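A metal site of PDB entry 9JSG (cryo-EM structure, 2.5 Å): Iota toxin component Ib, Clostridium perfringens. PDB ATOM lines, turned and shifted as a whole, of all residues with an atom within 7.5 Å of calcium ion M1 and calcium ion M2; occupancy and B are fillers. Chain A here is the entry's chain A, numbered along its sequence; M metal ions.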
ATOM      1  N   LEU A  18     -15.841  -8.234 -20.314  1.00  0.00           N
ATOM      2  CA  LEU A  18     -15.558  -7.717 -18.990  1.00  0.00           C
ATOM      3  C   LEU A  18     -16.837  -7.602 -18.181  1.00  0.00           C
ATOM      4  O   LEU A  18     -17.851  -7.082 -18.673  1.00  0.00           O
ATOM      5  CB  LEU A  18     -14.876  -6.349 -19.101  1.00  0.00           C
ATOM      6  CG  LEU A  18     -14.171  -5.842 -17.840  1.00  0.00           C
ATOM      7  CD1 LEU A  18     -13.003  -6.740 -17.465  1.00  0.00           C
ATOM      8  CD2 LEU A  18     -13.727  -4.402 -18.019  1.00  0.00           C
ATOM      9  N   ASP A  19     -16.804  -8.096 -16.947  1.00  0.00           N
ATOM     10  CA  ASP A  19     -17.933  -8.067 -16.025  1.00  0.00           C
ATOM     11  C   ASP A  19     -17.433  -7.513 -14.693  1.00  0.00           C
ATOM     12  O   ASP A  19     -16.928  -8.264 -13.852  1.00  0.00           O
ATOM     13  CB  ASP A  19     -18.560  -9.450 -15.869  1.00  0.00           C
ATOM     14  CG  ASP A  19     -19.943  -9.391 -15.270  1.00  0.00           C
ATOM     15  OD1 ASP A  19     -20.490  -8.277 -15.116  1.00  0.00           O
ATOM     16  OD2 ASP A  19     -20.504 -10.468 -14.951  1.00  0.00           O
ATOM     17  N   THR A  20     -17.558  -6.196 -14.515  1.00  0.00           N
ATOM     18  CA  THR A  20     -17.006  -5.554 -13.326  1.00  0.00           C
ATOM     19  C   THR A  20     -17.770  -5.940 -12.065  1.00  0.00           C
ATOM     20  O   THR A  20     -17.165  -6.264 -11.038  1.00  0.00           O
ATOM     21  CB  THR A  20     -16.998  -4.039 -13.507  1.00  0.00           C
ATOM     22  OG1 THR A  20     -16.480  -3.709 -14.803  1.00  0.00           O
ATOM     23  CG2 THR A  20     -16.147  -3.370 -12.437  1.00  0.00           C
ATOM     24  N   ASP A  21     -19.097  -5.917 -12.120  1.00  0.00           N
ATOM     25  CA  ASP A  21     -19.920  -6.192 -10.953  1.00  0.00           C
ATOM     26  C   ASP A  21     -20.260  -7.668 -10.792  1.00  0.00           C
ATOM     27  O   ASP A  21     -20.942  -8.031  -9.825  1.00  0.00           O
ATOM     28  CB  ASP A  21     -21.221  -5.377 -11.020  1.00  0.00           C
ATOM     29  CG  ASP A  21     -21.877  -5.445 -12.386  1.00  0.00           C
ATOM     30  OD1 ASP A  21     -21.262  -6.026 -13.307  1.00  0.00           O
ATOM     31  OD2 ASP A  21     -22.995  -4.915 -12.543  1.00  0.00           O
ATOM     32  N   ASN A  22     -19.769  -8.530 -11.692  1.00  0.00           N
ATOM     33  CA  ASN A  22     -20.047  -9.969 -11.655  1.00  0.00           C
ATOM     34  C   ASN A  22     -21.553 -10.248 -11.580  1.00  0.00           C
ATOM     35  O   ASN A  22     -22.002 -11.119 -10.842  1.00  0.00           O
ATOM     36  CB  ASN A  22     -19.312 -10.652 -10.499  1.00  0.00           C
ATOM     37  CG  ASN A  22     -17.925 -10.085 -10.267  1.00  0.00           C
ATOM     38  OD1 ASN A  22     -17.772  -9.047  -9.619  1.00  0.00           O
ATOM     39  ND2 ASN A  22     -16.903 -10.732 -10.821  1.00  0.00           N
ATOM     40  N   ASP A  23     -22.321  -9.502 -12.368  1.00  0.00           N
ATOM     41  CA  ASP A  23     -23.760  -9.667 -12.447  1.00  0.00           C
ATOM     42  C   ASP A  23     -24.174 -10.509 -13.655  1.00  0.00           C
ATOM     43  O   ASP A  23     -25.351 -10.514 -14.029  1.00  0.00           O
ATOM     44  CB  ASP A  23     -24.457  -8.304 -12.482  1.00  0.00           C
ATOM     45  CG  ASP A  23     -24.429  -7.671 -13.854  1.00  0.00           C
ATOM     46  OD1 ASP A  23     -23.339  -7.605 -14.465  1.00  0.00           O
ATOM     47  OD2 ASP A  23     -25.505  -7.227 -14.323  1.00  0.00           O
ATOM     48  N   ASN A  24     -23.220 -11.214 -14.269  1.00  0.00           N
ATOM     49  CA  ASN A  24     -23.397 -12.153 -15.382  1.00  0.00           C
ATOM     50  C   ASN A  24     -23.715 -11.466 -16.699  1.00  0.00           C
ATOM     51  O   ASN A  24     -24.045 -12.161 -17.680  1.00  0.00           O
ATOM     52  CB  ASN A  24     -24.455 -13.218 -15.081  1.00  0.00           C
ATOM     53  CG  ASN A  24     -23.902 -14.623 -15.110  1.00  0.00           C
ATOM     54  OD1 ASN A  24     -22.727 -14.841 -14.822  1.00  0.00           O
ATOM     55  ND2 ASN A  24     -24.754 -15.588 -15.453  1.00  0.00           N
ATOM     56  N   ILE A  25     -23.643 -10.144 -16.776  1.00  0.00           N
ATOM     57  CA  ILE A  25     -23.869  -9.399 -18.001  1.00  0.00           C
ATOM     58  C   ILE A  25     -22.637  -8.531 -18.259  1.00  0.00           C
ATOM     59  O   ILE A  25     -22.199  -7.821 -17.349  1.00  0.00           O
ATOM     60  CB  ILE A  25     -25.133  -8.528 -17.945  1.00  0.00           C
ATOM     61  CG1 ILE A  25     -26.307  -9.322 -17.377  1.00  0.00           C
ATOM     62  CG2 ILE A  25     -25.476  -7.983 -19.330  1.00  0.00           C
ATOM     63  CD1 ILE A  25     -27.355  -8.477 -16.676  1.00  0.00           C
ATOM     64  N   PRO A  26     -22.047  -8.572 -19.444  1.00  0.00           N
ATOM     65  CA  PRO A  26     -20.843  -7.772 -19.706  1.00  0.00           C
ATOM     66  C   PRO A  26     -21.128  -6.272 -19.632  1.00  0.00           C
ATOM     67  O   PRO A  26     -22.260  -5.823 -19.854  1.00  0.00           O
ATOM     68  CB  PRO A  26     -20.432  -8.188 -21.117  1.00  0.00           C
ATOM     69  CG  PRO A  26     -21.064  -9.530 -21.324  1.00  0.00           C
ATOM     70  CD  PRO A  26     -22.356  -9.485 -20.568  1.00  0.00           C
ATOM     71  N   ASP A  27     -20.087  -5.508 -19.308  1.00  0.00           N
ATOM     72  CA  ASP A  27     -20.228  -4.067 -19.156  1.00  0.00           C
ATOM     73  C   ASP A  27     -20.655  -3.406 -20.465  1.00  0.00           C
ATOM     74  O   ASP A  27     -21.496  -2.493 -20.460  1.00  0.00           O
ATOM     75  CB  ASP A  27     -18.914  -3.458 -18.665  1.00  0.00           C
ATOM     76  CG  ASP A  27     -18.434  -4.081 -17.373  1.00  0.00           C
ATOM     77  OD1 ASP A  27     -19.147  -4.948 -16.823  1.00  0.00           O
ATOM     78  OD2 ASP A  27     -17.330  -3.723 -16.918  1.00  0.00           O
ATOM     79  N   ALA A  28     -20.083  -3.838 -21.595  1.00  0.00           N
ATOM     80  CA  ALA A  28     -20.474  -3.275 -22.880  1.00  0.00           C
ATOM     81  C   ALA A  28     -21.929  -3.583 -23.200  1.00  0.00           C
ATOM     82  O   ALA A  28     -22.621  -2.772 -23.819  1.00  0.00           O
ATOM     83  CB  ALA A  28     -19.548  -3.811 -23.981  1.00  0.00           C
ATOM     84  N   TYR A  29     -22.408  -4.764 -22.779  1.00  0.00           N
ATOM     85  CA  TYR A  29     -23.803  -5.111 -23.006  1.00  0.00           C
ATOM     86  C   TYR A  29     -24.731  -4.258 -22.171  1.00  0.00           C
ATOM     87  O   TYR A  29     -25.839  -3.914 -22.602  1.00  0.00           O
ATOM     88  CB  TYR A  29     -24.027  -6.598 -22.707  1.00  0.00           C
ATOM     89  CG  TYR A  29     -23.492  -7.540 -23.767  1.00  0.00           C
ATOM     90  CD1 TYR A  29     -22.699  -7.070 -24.810  1.00  0.00           C
ATOM     91  CD2 TYR A  29     -23.772  -8.904 -23.717  1.00  0.00           C
ATOM     92  CE1 TYR A  29     -22.206  -7.933 -25.774  1.00  0.00           C
ATOM     93  CE2 TYR A  29     -23.287  -9.764 -24.675  1.00  0.00           C
ATOM     94  CZ  TYR A  29     -22.500  -9.279 -25.700  1.00  0.00           C
ATOM     95  N   GLU A  30     -24.310  -3.894 -20.954  1.00  0.00           N
ATOM     96  CA  GLU A  30     -25.152  -3.065 -20.085  1.00  0.00           C
ATOM     97  C   GLU A  30     -25.148  -1.604 -20.516  1.00  0.00           C
ATOM     98  O   GLU A  30     -26.170  -0.927 -20.432  1.00  0.00           O
ATOM     99  CB  GLU A  30     -24.709  -3.193 -18.628  1.00  0.00           C
ATOM    100  CG  GLU A  30     -24.718  -4.615 -18.103  1.00  0.00           C
ATOM    101  CD  GLU A  30     -24.778  -4.675 -16.597  1.00  0.00           C
ATOM    102  OE1 GLU A  30     -25.765  -4.167 -16.018  1.00  0.00           O
ATOM    103  OE2 GLU A  30     -23.846  -5.227 -15.976  1.00  0.00           O
ATOM    104  N   TYR A  34     -29.201  -4.895 -24.498  1.00  0.00           N
ATOM    105  CA  TYR A  34     -28.965  -6.327 -24.483  1.00  0.00           C
ATOM    106  C   TYR A  34     -30.290  -7.038 -24.281  1.00  0.00           C
ATOM    107  O   TYR A  34     -31.276  -6.441 -23.843  1.00  0.00           O
ATOM    108  CB  TYR A  34     -27.953  -6.719 -23.393  1.00  0.00           C
ATOM    109  CG  TYR A  34     -28.454  -6.531 -21.974  1.00  0.00           C
ATOM    110  CD1 TYR A  34     -28.327  -5.301 -21.332  1.00  0.00           C
ATOM    111  CD2 TYR A  34     -29.048  -7.575 -21.275  1.00  0.00           C
ATOM    112  CE1 TYR A  34     -28.776  -5.128 -20.043  1.00  0.00           C
ATOM    113  CE2 TYR A  34     -29.498  -7.411 -19.984  1.00  0.00           C
ATOM    114  CZ  TYR A  34     -29.367  -6.176 -19.371  1.00  0.00           C
ATOM    115  N   SER A  58     -28.794  -1.264 -18.047  1.00  0.00           N
ATOM    116  CA  SER A  58     -28.566  -1.274 -16.600  1.00  0.00           C
ATOM    117  C   SER A  58     -27.161  -0.735 -16.332  1.00  0.00           C
ATOM    118  O   SER A  58     -26.382  -0.480 -17.260  1.00  0.00           O
ATOM    119  CB  SER A  58     -28.748  -2.678 -16.017  1.00  0.00           C
ATOM    120  OG  SER A  58     -28.330  -3.675 -16.948  1.00  0.00           O
ATOM    121  N   SER A  59     -26.852  -0.564 -15.051  1.00  0.00           N
ATOM    122  CA  SER A  59     -25.556  -0.055 -14.621  1.00  0.00           C
ATOM    123  C   SER A  59     -24.546  -1.197 -14.591  1.00  0.00           C
ATOM    124  O   SER A  59     -24.814  -2.248 -13.994  1.00  0.00           O
ATOM    125  CB  SER A  59     -25.658   0.608 -13.250  1.00  0.00           C
ATOM    126  OG  SER A  59     -24.389   1.032 -12.798  1.00  0.00           O
ATOM    127  N   TYR A  60     -23.397  -0.992 -15.224  1.00  0.00           N
ATOM    128  CA  TYR A  60     -22.355  -2.005 -15.246  1.00  0.00           C
ATOM    129  C   TYR A  60     -21.510  -2.006 -13.977  1.00  0.00           C
ATOM    130  O   TYR A  60     -20.649  -2.885 -13.819  1.00  0.00           O
ATOM    131  CB  TYR A  60     -21.453  -1.820 -16.473  1.00  0.00           C
ATOM    132  CG  TYR A  60     -20.513  -0.643 -16.403  1.00  0.00           C
ATOM    133  CD1 TYR A  60     -20.927   0.632 -16.761  1.00  0.00           C
ATOM    134  CD2 TYR A  60     -19.191  -0.798 -15.989  1.00  0.00           C
ATOM    135  CE1 TYR A  60     -20.070   1.711 -16.701  1.00  0.00           C
ATOM    136  CE2 TYR A  60     -18.331   0.272 -15.920  1.00  0.00           C
ATOM    137  CZ  TYR A  60     -18.768   1.530 -16.284  1.00  0.00           C
ATOM    138  N   LEU A  61     -21.715  -1.051 -13.074  1.00  0.00           N
ATOM    139  CA  LEU A  61     -21.022  -1.007 -11.800  1.00  0.00           C
ATOM    140  C   LEU A  61     -21.901  -1.446 -10.628  1.00  0.00           C
ATOM    141  O   LEU A  61     -21.395  -1.545  -9.512  1.00  0.00           O
ATOM    142  CB  LEU A  61     -20.496   0.403 -11.523  1.00  0.00           C
ATOM    143  CG  LEU A  61     -19.207   0.809 -12.254  1.00  0.00           C
ATOM    144  CD1 LEU A  61     -18.824   2.240 -11.916  1.00  0.00           C
ATOM    145  CD2 LEU A  61     -18.074  -0.149 -11.915  1.00  0.00           C
ATOM    146  N   GLU A  62     -23.185  -1.715 -10.866  1.00  0.00           N
ATOM    147  CA  GLU A  62     -24.114  -2.134  -9.819  1.00  0.00           C
ATOM    148  C   GLU A  62     -24.760  -3.437 -10.232  1.00  0.00           C
ATOM    149  O   GLU A  62     -25.313  -3.534 -11.335  1.00  0.00           O
ATOM    150  CB  GLU A  62     -25.176  -1.054  -9.566  1.00  0.00           C
ATOM    151  CG  GLU A  62     -25.493  -0.826  -8.101  1.00  0.00           C
ATOM    152  CD  GLU A  62     -24.271  -0.421  -7.295  1.00  0.00           C
ATOM    153  OE1 GLU A  62     -23.603   0.557  -7.684  1.00  0.00           O
ATOM    154  OE2 GLU A  62     -23.992  -1.081  -6.278  1.00  0.00           O
ATOM    155  N   SER A  63     -24.701  -4.437  -9.357  1.00  0.00           N
ATOM    156  CA  SER A  63     -25.354  -5.716  -9.638  1.00  0.00           C
ATOM    157  C   SER A  63     -26.866  -5.607  -9.498  1.00  0.00           C
ATOM    158  O   SER A  63     -27.615  -6.306 -10.203  1.00  0.00           O
ATOM    159  CB  SER A  63     -24.802  -6.808  -8.730  1.00  0.00           C
ATOM    160  OG  SER A  63     -25.315  -6.689  -7.416  1.00  0.00           O
ATOM    161  N   ASN A  64     -27.346  -4.758  -8.595  1.00  0.00           N
ATOM    162  CA  ASN A  64     -28.762  -4.511  -8.377  1.00  0.00           C
ATOM    163  C   ASN A  64     -29.010  -3.026  -8.637  1.00  0.00           C
ATOM    164  O   ASN A  64     -28.896  -2.195  -7.741  1.00  0.00           O
ATOM    165  CB  ASN A  64     -29.201  -4.910  -6.965  1.00  0.00           C
ATOM    166  CG  ASN A  64     -28.883  -6.368  -6.645  1.00  0.00           C
ATOM    167  OD1 ASN A  64     -27.754  -6.811  -6.802  1.00  0.00           O
ATOM    168  ND2 ASN A  64     -29.897  -7.104  -6.203  1.00  0.00           N
ATOM    169  N   THR A  65     -29.335  -2.702  -9.896  1.00  0.00           N
ATOM    170  CA  THR A  65     -29.509  -1.297 -10.277  1.00  0.00           C
ATOM    171  C   THR A  65     -30.688  -0.657  -9.549  1.00  0.00           C
ATOM    172  O   THR A  65     -30.586   0.475  -9.077  1.00  0.00           O
ATOM    173  CB  THR A  65     -29.688  -1.195 -11.788  1.00  0.00           C
ATOM    174  OG1 THR A  65     -28.546  -1.752 -12.449  1.00  0.00           O
ATOM    175  CG2 THR A  65     -29.846   0.262 -12.206  1.00  0.00           C
ATOM    176  N   THR A  71     -31.002  -9.317  -8.778  1.00  0.00           N
ATOM    177  CA  THR A  71     -29.986  -8.713  -9.614  1.00  0.00           C
ATOM    178  C   THR A  71     -30.546  -8.423 -11.007  1.00  0.00           C
ATOM    179  O   THR A  71     -31.651  -8.825 -11.359  1.00  0.00           O
ATOM    180  CB  THR A  71     -28.758  -9.616  -9.719  1.00  0.00           C
ATOM    181  OG1 THR A  71     -29.026 -10.687 -10.632  1.00  0.00           O
ATOM    182  CG2 THR A  71     -28.404 -10.199  -8.354  1.00  0.00           C
ATOM    183  N   ASP A  72     -29.747  -7.702 -11.802  1.00  0.00           N
ATOM    184  CA  ASP A  72     -30.179  -7.316 -13.142  1.00  0.00           C
ATOM    185  C   ASP A  72     -30.409  -8.545 -14.020  1.00  0.00           C
ATOM    186  O   ASP A  72     -31.412  -8.620 -14.747  1.00  0.00           O
ATOM    187  CB  ASP A  72     -29.144  -6.390 -13.780  1.00  0.00           C
ATOM    188  CG  ASP A  72     -29.010  -5.080 -13.030  1.00  0.00           C
ATOM    189  OD1 ASP A  72     -29.997  -4.646 -12.400  1.00  0.00           O
ATOM    190  OD2 ASP A  72     -27.917  -4.479 -13.089  1.00  0.00           O
ATOM    191  N   TYR A  73     -29.490  -9.511 -13.984  1.00  0.00           N
ATOM    192  CA  TYR A  73     -29.645 -10.713 -14.795  1.00  0.00           C
ATOM    193  C   TYR A  73     -30.845 -11.543 -14.346  1.00  0.00           C
ATOM    194  O   TYR A  73     -31.564 -12.105 -15.177  1.00  0.00           O
ATOM    195  CB  TYR A  73     -28.369 -11.557 -14.747  1.00  0.00           C
ATOM    196  CG  TYR A  73     -28.483 -12.870 -15.487  1.00  0.00           C
ATOM    197  CD1 TYR A  73     -28.388 -12.909 -16.869  1.00  0.00           C
ATOM    198  CD2 TYR A  73     -28.696 -14.063 -14.805  1.00  0.00           C
ATOM    199  CE1 TYR A  73     -28.495 -14.110 -17.551  1.00  0.00           C
ATOM    200  CE2 TYR A  73     -28.797 -15.263 -15.480  1.00  0.00           C
ATOM    201  CZ  TYR A  73     -28.700 -15.280 -16.851  1.00  0.00           C
ATOM    202  N   PRO A  91     -34.644  -4.085 -15.574  1.00  0.00           N
ATOM    203  CA  PRO A  91     -33.734  -3.725 -14.472  1.00  0.00           C
ATOM    204  C   PRO A  91     -34.006  -2.361 -13.862  1.00  0.00           C
ATOM    205  O   PRO A  91     -33.711  -2.153 -12.684  1.00  0.00           O
ATOM    206  CB  PRO A  91     -32.340  -3.776 -15.130  1.00  0.00           C
ATOM    207  CG  PRO A  91     -32.519  -4.666 -16.318  1.00  0.00           C
ATOM    208  CD  PRO A  91     -33.910  -4.407 -16.818  1.00  0.00           C
HETATM  209 CA    CA M   1     -25.335  -4.675 -13.558  1.00  0.00          CA
HETATM  210 CA    CA M   2     -21.539  -6.058 -15.744  1.00  0.00          CA
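The side-chain carboxylate of Asp 72 is in hydrogen-bond range of the side-chain hydroxyl of Thr 65.
The side-chain carboxylate (OD2) of Asp 19 sits at hydrogen-bond distance from the backbone NH (N) of Asn 24.
The backbone NH (N) of Thr 20 lies close to the side-chain carboxylate (OD2) of Asp 27, 3.5 Å away.
OG of Ser 59 lies close to N of Leu 61 (3.4 Å).
N of Ser 59 sits at hydrogen-bond distance from OG1 of Thr 65 (3.3 Å).
N of Asp 72 sits at hydrogen-bond distance from O of Ser 63 (3.0 Å).
The backbone NH (N) of Asp 27 lies within hydrogen-bond range of the backbone carbonyl oxygen (O) of Leu 18 (2.8 Å).
The side-chain carboxylate of Glu 30 lies close to the side-chain hydroxyl of Ser 58 (2.8 Å).
Pro 26 touches calcium ion M2 (C to CA, 3.9 Å).
O of Tyr 60 touches calcium ion M2 (3.8 Å).
Of the 26 residues printed, 8 come within 4 Å of calcium ion M2.
Calcium ion M1 is bound by O of Glu 62, O of Ser 59, OE1 of Glu 30, OD2 of Asp 21, OD2 of Asp 72, OD2 of Asp 23 and OE2 of Glu 30.
Calcium ion M1 has seven donor atoms within binding distance.
Calcium ion M2 is bound by the side-chain carboxylate of Asp 21 (2.5 Å), the side-chain carboxylate of Glu 30 (2.5 Å), the backbone carbonyl oxygen of Ile 25 (2.5 Å), the side-chain carboxylate of Asp 19 (2.5 Å), the side-chain carboxylate of Asp 23 (2.7 Å) and the side-chain carboxylate of Asp 27 (2.8 Å).
Calcium ion M2 has six donor atoms within binding distance.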
